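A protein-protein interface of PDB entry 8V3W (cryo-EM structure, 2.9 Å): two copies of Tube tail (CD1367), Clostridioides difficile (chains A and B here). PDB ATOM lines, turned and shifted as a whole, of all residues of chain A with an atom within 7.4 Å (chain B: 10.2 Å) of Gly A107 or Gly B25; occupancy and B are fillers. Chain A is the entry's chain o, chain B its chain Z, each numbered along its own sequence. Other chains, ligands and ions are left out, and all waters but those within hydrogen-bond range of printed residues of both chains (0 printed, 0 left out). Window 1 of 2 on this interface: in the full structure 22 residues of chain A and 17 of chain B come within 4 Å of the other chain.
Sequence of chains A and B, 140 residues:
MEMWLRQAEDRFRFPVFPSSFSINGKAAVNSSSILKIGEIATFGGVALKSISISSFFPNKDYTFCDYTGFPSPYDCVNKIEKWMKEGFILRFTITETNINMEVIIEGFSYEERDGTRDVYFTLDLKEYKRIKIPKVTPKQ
N of Ile B23 lies within hydrogen-bond range of O of Tyr A110 (3.0 Å). The backbone carbonyl oxygen (O) of Phe A108 sits at hydrogen-bond distance from the backbone NH (N) of Gly B25, 3.1 Å away. The backbone carbonyl oxygen (O) of Glu A106 lies within hydrogen-bond range of the backbone NH (N) of Ala B27 (2.9 Å). NZ of Lys B49 lies within salt-bridge range of OE2 of Glu A81.
The backbone carbonyl oxygen of Ser B50 sits at hydrogen-bond distance from the backbone NH of Asn B24 (3.2 Å). O of Lys B26 sits at hydrogen-bond distance from N of Ala B47 (3.2 Å). The backbone carbonyl oxygen (O) of Lys B49 sits at hydrogen-bond distance from the backbone NH (N) of Glu B127 (3.1 Å). The backbone carbonyl oxygen (O) of Asp A124 sits at hydrogen-bond distance from the backbone NH (N) of Glu A106 (2.9 Å). O of Gly A107 is in hydrogen-bond range of N of Asp A124 (3.1 Å). The backbone NH of Thr A122 sits at hydrogen-bond distance from the backbone carbonyl oxygen of Ser A109, 3.0 Å away.
Among the printed residues, pairs that only touch across the chains: Ser A109 with Ile B23, Tyr A110 with Ser B22, Gly A107 with Gly B25, Ser A109 with Asn B24, Glu A106 with Lys B26, Met A84 with Lys B26, Ile A104 with Phe B43, Ser A109 with Gly B25, Met A84 with Gly B25 and Ile A105 with Ala B27.
Of the printed residues of chain B, Gly A107 touches Gly B25. Of the printed residues of chain A, Gly B25 touches Met A84, Gly A107, Phe A108 and Ser A109. No residue of chain B comes within 4 Å of Leu A123. No residue of chain B comes within 4 Å of Asp A124. Of the printed residues of chain A, Ala B27 touches Ile A105 and Glu A106. Of the printed residues of chain B, Tyr A110 touches Ser B22 (3.4 Å) and Ile B23 (3.0 Å). Val B46 touches none of the printed residues of chain A. The nearest printed residue of chain B that does not touch Gly A107 is Lys B26 (4.005 Å). The nearest residue of chain A that does not touch Gly B25 is Glu A106 (4.7 Å). The nearest printed residue of chain A that does not touch Lys B49 is Tyr A110 (4.4 Å).
Printed residues of chain A that touch a printed residue of chain B: Glu A81, Met A84, Ile A104, Ile A105, Glu A106, Gly A107, Phe A108, Ser A109 and Tyr A110. Hydrophobic or aromatic side chains of chain A within 4 Å of the printed part of chain B: Met A84, Ile A104 and Tyr A110. Of the 18 printed residues of chain B, 8 touch a printed residue of chain A. Hydrophobic or aromatic side chains of chain B within 4 Å of the printed part of chain A: Ile B23, Ala B27 and Phe B43.
No position is printed for both chains.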
ATOM      1  N   ILE A  80      19.814  11.583  36.417  1.00  0.00           N
ATOM      2  CA  ILE A  80      21.258  11.744  36.280  1.00  0.00           C
ATOM      3  C   ILE A  80      21.620  12.254  34.890  1.00  0.00           C
ATOM      4  O   ILE A  80      22.545  13.061  34.733  1.00  0.00           O
ATOM      5  CB  ILE A  80      21.977  10.429  36.621  1.00  0.00           C
ATOM      6  CG1 ILE A  80      21.689  10.044  38.067  1.00  0.00           C
ATOM      7  CG2 ILE A  80      23.473  10.571  36.428  1.00  0.00           C
ATOM      8  CD1 ILE A  80      22.216   8.702  38.450  1.00  0.00           C
ATOM      9  N   GLU A  81      20.900  11.807  33.860  1.00  0.00           N
ATOM     10  CA  GLU A  81      21.176  12.279  32.508  1.00  0.00           C
ATOM     11  C   GLU A  81      20.891  13.765  32.364  1.00  0.00           C
ATOM     12  O   GLU A  81      21.650  14.483  31.707  1.00  0.00           O
ATOM     13  CB  GLU A  81      20.362  11.484  31.496  1.00  0.00           C
ATOM     14  CG  GLU A  81      21.146  10.412  30.785  1.00  0.00           C
ATOM     15  CD  GLU A  81      20.634  10.161  29.388  1.00  0.00           C
ATOM     16  OE1 GLU A  81      19.409  10.259  29.178  1.00  0.00           O
ATOM     17  OE2 GLU A  81      21.456   9.872  28.497  1.00  0.00           O
ATOM     18  N   MET A  84      23.765  15.621  33.967  1.00  0.00           N
ATOM     19  CA  MET A  84      24.964  15.601  33.134  1.00  0.00           C
ATOM     20  C   MET A  84      24.821  16.524  31.933  1.00  0.00           C
ATOM     21  O   MET A  84      25.784  17.187  31.535  1.00  0.00           O
ATOM     22  CB  MET A  84      25.271  14.176  32.677  1.00  0.00           C
ATOM     23  CG  MET A  84      26.506  14.059  31.804  1.00  0.00           C
ATOM     24  SD  MET A  84      26.908  12.371  31.334  1.00  0.00           S
ATOM     25  CE  MET A  84      26.365  12.351  29.637  1.00  0.00           C
ATOM     26  N   ILE A 104      31.566  17.335  39.078  1.00  0.00           N
ATOM     27  CA  ILE A 104      30.868  17.532  37.814  1.00  0.00           C
ATOM     28  C   ILE A 104      30.937  16.222  37.036  1.00  0.00           C
ATOM     29  O   ILE A 104      31.950  15.517  37.079  1.00  0.00           O
ATOM     30  CB  ILE A 104      31.459  18.717  37.019  1.00  0.00           C
ATOM     31  CG1 ILE A 104      30.480  19.192  35.950  1.00  0.00           C
ATOM     32  CG2 ILE A 104      32.801  18.370  36.410  1.00  0.00           C
ATOM     33  CD1 ILE A 104      30.892  20.477  35.293  1.00  0.00           C
ATOM     34  N   ILE A 105      29.851  15.874  36.356  1.00  0.00           N
ATOM     35  CA  ILE A 105      29.734  14.559  35.731  1.00  0.00           C
ATOM     36  C   ILE A 105      30.441  14.560  34.382  1.00  0.00           C
ATOM     37  O   ILE A 105      30.260  15.473  33.572  1.00  0.00           O
ATOM     38  CB  ILE A 105      28.259  14.154  35.583  1.00  0.00           C
ATOM     39  CG1 ILE A 105      27.590  14.087  36.950  1.00  0.00           C
ATOM     40  CG2 ILE A 105      28.138  12.809  34.905  1.00  0.00           C
ATOM     41  CD1 ILE A 105      26.109  13.870  36.888  1.00  0.00           C
ATOM     42  N   GLU A 106      31.248  13.527  34.139  1.00  0.00           N
ATOM     43  CA  GLU A 106      32.024  13.386  32.914  1.00  0.00           C
ATOM     44  C   GLU A 106      31.500  12.317  31.971  1.00  0.00           C
ATOM     45  O   GLU A 106      31.637  12.469  30.759  1.00  0.00           O
ATOM     46  CB  GLU A 106      33.480  13.057  33.246  1.00  0.00           C
ATOM     47  CG  GLU A 106      34.421  14.227  33.189  1.00  0.00           C
ATOM     48  CD  GLU A 106      35.867  13.782  33.176  1.00  0.00           C
ATOM     49  OE1 GLU A 106      36.230  12.927  34.011  1.00  0.00           O
ATOM     50  OE2 GLU A 106      36.640  14.281  32.332  1.00  0.00           O
ATOM     51  N   GLY A 107      30.922  11.239  32.488  1.00  0.00           N
ATOM     52  CA  GLY A 107      30.403  10.188  31.635  1.00  0.00           C
ATOM     53  C   GLY A 107      29.349   9.383  32.352  1.00  0.00           C
ATOM     54  O   GLY A 107      29.381   9.241  33.576  1.00  0.00           O
ATOM     55  N   PHE A 108      28.411   8.844  31.579  1.00  0.00           N
ATOM     56  CA  PHE A 108      27.319   8.046  32.124  1.00  0.00           C
ATOM     57  C   PHE A 108      26.897   7.026  31.082  1.00  0.00           C
ATOM     58  O   PHE A 108      26.497   7.402  29.978  1.00  0.00           O
ATOM     59  CB  PHE A 108      26.139   8.934  32.514  1.00  0.00           C
ATOM     60  CG  PHE A 108      25.086   8.229  33.314  1.00  0.00           C
ATOM     61  CD1 PHE A 108      25.427   7.463  34.412  1.00  0.00           C
ATOM     62  CD2 PHE A 108      23.755   8.337  32.974  1.00  0.00           C
ATOM     63  CE1 PHE A 108      24.461   6.818  35.149  1.00  0.00           C
ATOM     64  CE2 PHE A 108      22.787   7.692  33.708  1.00  0.00           C
ATOM     65  CZ  PHE A 108      23.140   6.931  34.792  1.00  0.00           C
ATOM     66  N   SER A 109      26.972   5.747  31.430  1.00  0.00           N
ATOM     67  CA  SER A 109      26.577   4.662  30.546  1.00  0.00           C
ATOM     68  C   SER A 109      25.721   3.672  31.318  1.00  0.00           C
ATOM     69  O   SER A 109      25.986   3.405  32.491  1.00  0.00           O
ATOM     70  CB  SER A 109      27.796   3.948  29.967  1.00  0.00           C
ATOM     71  OG  SER A 109      28.629   4.847  29.262  1.00  0.00           O
ATOM     72  N   TYR A 110      24.703   3.122  30.661  1.00  0.00           N
ATOM     73  CA  TYR A 110      23.812   2.168  31.302  1.00  0.00           C
ATOM     74  C   TYR A 110      23.418   1.081  30.312  1.00  0.00           C
ATOM     75  O   TYR A 110      23.501   1.265  29.098  1.00  0.00           O
ATOM     76  CB  TYR A 110      22.567   2.852  31.876  1.00  0.00           C
ATOM     77  CG  TYR A 110      21.848   3.772  30.923  1.00  0.00           C
ATOM     78  CD1 TYR A 110      22.297   5.062  30.694  1.00  0.00           C
ATOM     79  CD2 TYR A 110      20.701   3.359  30.266  1.00  0.00           C
ATOM     80  CE1 TYR A 110      21.636   5.899  29.834  1.00  0.00           C
ATOM     81  CE2 TYR A 110      20.038   4.191  29.406  1.00  0.00           C
ATOM     82  CZ  TYR A 110      20.508   5.460  29.194  1.00  0.00           C
ATOM     83  OH  TYR A 110      19.848   6.300  28.332  1.00  0.00           O
ATOM     84  N   THR A 122      27.557   2.894  34.951  1.00  0.00           N
ATOM     85  CA  THR A 122      28.879   3.373  35.336  1.00  0.00           C
ATOM     86  C   THR A 122      28.881   4.892  35.278  1.00  0.00           C
ATOM     87  O   THR A 122      28.491   5.473  34.263  1.00  0.00           O
ATOM     88  CB  THR A 122      29.977   2.816  34.425  1.00  0.00           C
ATOM     89  OG1 THR A 122      29.960   1.386  34.467  1.00  0.00           O
ATOM     90  CG2 THR A 122      31.341   3.301  34.878  1.00  0.00           C
ATOM     91  N   LEU A 123      29.335   5.528  36.353  1.00  0.00           N
ATOM     92  CA  LEU A 123      29.313   6.979  36.493  1.00  0.00           C
ATOM     93  C   LEU A 123      30.718   7.494  36.766  1.00  0.00           C
ATOM     94  O   LEU A 123      31.394   7.001  37.671  1.00  0.00           O
ATOM     95  CB  LEU A 123      28.366   7.382  37.625  1.00  0.00           C
ATOM     96  CG  LEU A 123      28.097   8.850  37.933  1.00  0.00           C
ATOM     97  CD1 LEU A 123      27.353   9.518  36.806  1.00  0.00           C
ATOM     98  CD2 LEU A 123      27.303   8.943  39.210  1.00  0.00           C
ATOM     99  N   ASP A 124      31.151   8.488  35.994  1.00  0.00           N
ATOM    100  CA  ASP A 124      32.461   9.110  36.148  1.00  0.00           C
ATOM    101  C   ASP A 124      32.299  10.541  36.636  1.00  0.00           C
ATOM    102  O   ASP A 124      31.608  11.341  35.999  1.00  0.00           O
ATOM    103  CB  ASP A 124      33.233   9.102  34.827  1.00  0.00           C
ATOM    104  CG  ASP A 124      33.344   7.721  34.223  1.00  0.00           C
ATOM    105  OD1 ASP A 124      32.855   6.756  34.839  1.00  0.00           O
ATOM    106  OD2 ASP A 124      33.933   7.593  33.131  1.00  0.00           O
ATOM    107  N   LEU A 125      32.951  10.869  37.747  1.00  0.00           N
ATOM    108  CA  LEU A 125      32.854  12.182  38.363  1.00  0.00           C
ATOM    109  C   LEU A 125      34.233  12.815  38.480  1.00  0.00           C
ATOM    110  O   LEU A 125      35.236  12.125  38.665  1.00  0.00           O
ATOM    111  CB  LEU A 125      32.209  12.097  39.746  1.00  0.00           C
ATOM    112  CG  LEU A 125      30.939  11.255  39.843  1.00  0.00           C
ATOM    113  CD1 LEU A 125      30.598  10.963  41.287  1.00  0.00           C
ATOM    114  CD2 LEU A 125      29.785  11.948  39.155  1.00  0.00           C
ATOM    115  N   LYS A 126      34.274  14.138  38.361  1.00  0.00           N
ATOM    116  CA  LYS A 126      35.511  14.897  38.452  1.00  0.00           C
ATOM    117  C   LYS A 126      35.332  16.030  39.449  1.00  0.00           C
ATOM    118  O   LYS A 126      34.293  16.689  39.466  1.00  0.00           O
ATOM    119  CB  LYS A 126      35.922  15.466  37.095  1.00  0.00           C
ATOM    120  CG  LYS A 126      37.369  15.897  37.023  1.00  0.00           C
ATOM    121  CD  LYS A 126      37.676  16.569  35.706  1.00  0.00           C
ATOM    122  CE  LYS A 126      39.160  16.561  35.418  1.00  0.00           C
ATOM    123  NZ  LYS A 126      39.630  15.198  35.069  1.00  0.00           N
ATOM    124  N   SER B  22      23.540  -1.371  25.312  1.00  0.00           N
ATOM    125  CA  SER B  22      24.133  -0.367  26.186  1.00  0.00           C
ATOM    126  C   SER B  22      24.233   0.978  25.483  1.00  0.00           C
ATOM    127  O   SER B  22      24.542   1.045  24.293  1.00  0.00           O
ATOM    128  CB  SER B  22      25.523  -0.797  26.666  1.00  0.00           C
ATOM    129  OG  SER B  22      26.355  -1.157  25.582  1.00  0.00           O
ATOM    130  N   ILE B  23      23.995   2.048  26.239  1.00  0.00           N
ATOM    131  CA  ILE B  23      24.032   3.420  25.743  1.00  0.00           C
ATOM    132  C   ILE B  23      25.219   4.130  26.380  1.00  0.00           C
ATOM    133  O   ILE B  23      25.374   4.105  27.605  1.00  0.00           O
ATOM    134  CB  ILE B  23      22.722   4.160  26.060  1.00  0.00           C
ATOM    135  CG1 ILE B  23      21.565   3.572  25.254  1.00  0.00           C
ATOM    136  CG2 ILE B  23      22.867   5.648  25.815  1.00  0.00           C
ATOM    137  CD1 ILE B  23      21.323   4.256  23.934  1.00  0.00           C
ATOM    138  N   ASN B  24      26.052   4.765  25.556  1.00  0.00           N
ATOM    139  CA  ASN B  24      27.235   5.482  26.020  1.00  0.00           C
ATOM    140  C   ASN B  24      27.019   6.986  25.923  1.00  0.00           C
ATOM    141  O   ASN B  24      26.603   7.490  24.878  1.00  0.00           O
ATOM    142  CB  ASN B  24      28.470   5.095  25.208  1.00  0.00           C
ATOM    143  CG  ASN B  24      28.738   3.608  25.220  1.00  0.00           C
ATOM    144  OD1 ASN B  24      29.141   3.045  26.236  1.00  0.00           O
ATOM    145  ND2 ASN B  24      28.528   2.962  24.081  1.00  0.00           N
ATOM    146  N   GLY B  25      27.326   7.696  27.001  1.00  0.00           N
ATOM    147  CA  GLY B  25      27.236   9.143  27.012  1.00  0.00           C
ATOM    148  C   GLY B  25      28.465   9.758  27.646  1.00  0.00           C
ATOM    149  O   GLY B  25      29.064   9.196  28.561  1.00  0.00           O
ATOM    150  N   LYS B  26      28.834  10.935  27.148  1.00  0.00           N
ATOM    151  CA  LYS B  26      30.028  11.627  27.612  1.00  0.00           C
ATOM    152  C   LYS B  26      29.779  13.127  27.653  1.00  0.00           C
ATOM    153  O   LYS B  26      28.837  13.640  27.049  1.00  0.00           O
ATOM    154  CB  LYS B  26      31.240  11.333  26.723  1.00  0.00           C
ATOM    155  CG  LYS B  26      31.814   9.948  26.903  1.00  0.00           C
ATOM    156  CD  LYS B  26      33.323   9.968  26.870  1.00  0.00           C
ATOM    157  CE  LYS B  26      33.891  10.372  28.220  1.00  0.00           C
ATOM    158  NZ  LYS B  26      33.550   9.394  29.289  1.00  0.00           N
ATOM    159  N   ALA B  27      30.634  13.826  28.395  1.00  0.00           N
ATOM    160  CA  ALA B  27      30.629  15.280  28.445  1.00  0.00           C
ATOM    161  C   ALA B  27      32.062  15.784  28.383  1.00  0.00           C
ATOM    162  O   ALA B  27      32.981  15.142  28.896  1.00  0.00           O
ATOM    163  CB  ALA B  27      29.943  15.805  29.709  1.00  0.00           C
ATOM    164  N   ALA B  28      32.247  16.941  27.756  1.00  0.00           N
ATOM    165  CA  ALA B  28      33.568  17.532  27.602  1.00  0.00           C
ATOM    166  C   ALA B  28      33.880  18.467  28.763  1.00  0.00           C
ATOM    167  O   ALA B  28      33.022  19.227  29.213  1.00  0.00           O
ATOM    168  CB  ALA B  28      33.664  18.291  26.280  1.00  0.00           C
ATOM    169  N   VAL B  29      35.118  18.405  29.241  1.00  0.00           N
ATOM    170  CA  VAL B  29      35.581  19.221  30.357  1.00  0.00           C
ATOM    171  C   VAL B  29      36.906  19.863  29.968  1.00  0.00           C
ATOM    172  O   VAL B  29      37.851  19.162  29.596  1.00  0.00           O
ATOM    173  CB  VAL B  29      35.734  18.386  31.642  1.00  0.00           C
ATOM    174  CG1 VAL B  29      36.681  19.058  32.606  1.00  0.00           C
ATOM    175  CG2 VAL B  29      34.381  18.160  32.286  1.00  0.00           C
ATOM    176  N   PHE B  43      32.840  23.233  32.497  1.00  0.00           N
ATOM    177  CA  PHE B  43      31.981  22.463  31.608  1.00  0.00           C
ATOM    178  C   PHE B  43      32.096  22.967  30.174  1.00  0.00           C
ATOM    179  O   PHE B  43      32.163  24.172  29.927  1.00  0.00           O
ATOM    180  CB  PHE B  43      30.537  22.551  32.090  1.00  0.00           C
ATOM    181  CG  PHE B  43      29.553  21.835  31.219  1.00  0.00           C
ATOM    182  CD1 PHE B  43      29.636  20.469  31.032  1.00  0.00           C
ATOM    183  CD2 PHE B  43      28.528  22.526  30.601  1.00  0.00           C
ATOM    184  CE1 PHE B  43      28.723  19.812  30.237  1.00  0.00           C
ATOM    185  CE2 PHE B  43      27.616  21.873  29.809  1.00  0.00           C
ATOM    186  CZ  PHE B  43      27.714  20.514  29.627  1.00  0.00           C
ATOM    187  N   GLY B  45      30.309  21.147  27.275  1.00  0.00           N
ATOM    188  CA  GLY B  45      29.276  20.674  26.374  1.00  0.00           C
ATOM    189  C   GLY B  45      29.175  19.165  26.305  1.00  0.00           C
ATOM    190  O   GLY B  45      30.147  18.460  26.579  1.00  0.00           O
ATOM    191  N   VAL B  46      28.012  18.658  25.917  1.00  0.00           N
ATOM    192  CA  VAL B  46      27.733  17.228  25.920  1.00  0.00           C
ATOM    193  C   VAL B  46      27.933  16.670  24.516  1.00  0.00           C
ATOM    194  O   VAL B  46      27.774  17.374  23.515  1.00  0.00           O
ATOM    195  CB  VAL B  46      26.304  16.960  26.445  1.00  0.00           C
ATOM    196  CG1 VAL B  46      25.268  17.334  25.408  1.00  0.00           C
ATOM    197  CG2 VAL B  46      26.147  15.519  26.873  1.00  0.00           C
ATOM    198  N   ALA B  47      28.299  15.393  24.439  1.00  0.00           N
ATOM    199  CA  ALA B  47      28.523  14.716  23.172  1.00  0.00           C
ATOM    200  C   ALA B  47      27.289  13.909  22.773  1.00  0.00           C
ATOM    201  O   ALA B  47      26.299  13.832  23.501  1.00  0.00           O
ATOM    202  CB  ALA B  47      29.756  13.819  23.255  1.00  0.00           C
ATOM    203  N   LEU B  48      27.352  13.300  21.592  1.00  0.00           N
ATOM    204  CA  LEU B  48      26.251  12.502  21.071  1.00  0.00           C
ATOM    205  C   LEU B  48      26.326  11.072  21.592  1.00  0.00           C
ATOM    206  O   LEU B  48      27.410  10.496  21.706  1.00  0.00           O
ATOM    207  CB  LEU B  48      26.264  12.494  19.542  1.00  0.00           C
ATOM    208  CG  LEU B  48      26.212  13.830  18.795  1.00  0.00           C
ATOM    209  CD1 LEU B  48      26.808  13.688  17.411  1.00  0.00           C
ATOM    210  CD2 LEU B  48      24.796  14.353  18.703  1.00  0.00           C
ATOM    211  N   LYS B  49      25.164  10.496  21.888  1.00  0.00           N
ATOM    212  CA  LYS B  49      25.105   9.123  22.360  1.00  0.00           C
ATOM    213  C   LYS B  49      25.392   8.145  21.227  1.00  0.00           C
ATOM    214  O   LYS B  49      25.204   8.444  20.048  1.00  0.00           O
ATOM    215  CB  LYS B  49      23.734   8.810  22.948  1.00  0.00           C
ATOM    216  CG  LYS B  49      23.225   9.813  23.944  1.00  0.00           C
ATOM    217  CD  LYS B  49      21.901   9.345  24.498  1.00  0.00           C
ATOM    218  CE  LYS B  49      21.221  10.422  25.299  1.00  0.00           C
ATOM    219  NZ  LYS B  49      19.951   9.922  25.877  1.00  0.00           N
ATOM    220  N   SER B  50      25.840   6.949  21.603  1.00  0.00           N
ATOM    221  CA  SER B  50      26.104   5.889  20.644  1.00  0.00           C
ATOM    222  C   SER B  50      25.571   4.568  21.180  1.00  0.00           C
ATOM    223  O   SER B  50      25.465   4.370  22.390  1.00  0.00           O
ATOM    224  CB  SER B  50      27.600   5.779  20.329  1.00  0.00           C
ATOM    225  OG  SER B  50      28.371   5.676  21.508  1.00  0.00           O
ATOM    226  N   ILE B  51      25.234   3.670  20.258  1.00  0.00           N
ATOM    227  CA  ILE B  51      24.590   2.398  20.574  1.00  0.00           C
ATOM    228  C   ILE B  51      24.999   1.375  19.522  1.00  0.00           C
ATOM    229  O   ILE B  51      25.048   1.682  18.330  1.00  0.00           O
ATOM    230  CB  ILE B  51      23.055   2.563  20.656  1.00  0.00           C
ATOM    231  CG1 ILE B  51      22.343   1.213  20.725  1.00  0.00           C
ATOM    232  CG2 ILE B  51      22.537   3.374  19.495  1.00  0.00           C
ATOM    233  CD1 ILE B  51      22.372   0.567  22.063  1.00  0.00           C
ATOM    234  N   MET B 101      14.831   7.934  19.830  1.00  0.00           N
ATOM    235  CA  MET B 101      15.561   9.081  19.308  1.00  0.00           C
ATOM    236  C   MET B 101      15.862   8.894  17.830  1.00  0.00           C
ATOM    237  O   MET B 101      15.755   7.794  17.286  1.00  0.00           O
ATOM    238  CB  MET B 101      16.861   9.307  20.078  1.00  0.00           C
ATOM    239  CG  MET B 101      17.905   8.242  19.845  1.00  0.00           C
ATOM    240  SD  MET B 101      19.300   8.405  20.965  1.00  0.00           S
ATOM    241  CE  MET B 101      20.142   6.857  20.675  1.00  0.00           C
ATOM    242  N   GLU B 127      23.551   9.259  17.562  1.00  0.00           N
ATOM    243  CA  GLU B 127      22.495  10.242  17.755  1.00  0.00           C
ATOM    244  C   GLU B 127      22.656  11.400  16.779  1.00  0.00           C
ATOM    245  O   GLU B 127      23.771  11.798  16.439  1.00  0.00           O
ATOM    246  CB  GLU B 127      22.517  10.755  19.193  1.00  0.00           C
ATOM    247  CG  GLU B 127      21.367  11.674  19.554  1.00  0.00           C
ATOM    248  CD  GLU B 127      21.587  12.397  20.867  1.00  0.00           C
ATOM    249  OE1 GLU B 127      22.740  12.440  21.343  1.00  0.00           O
ATOM    250  OE2 GLU B 127      20.607  12.928  21.424  1.00  0.00           O
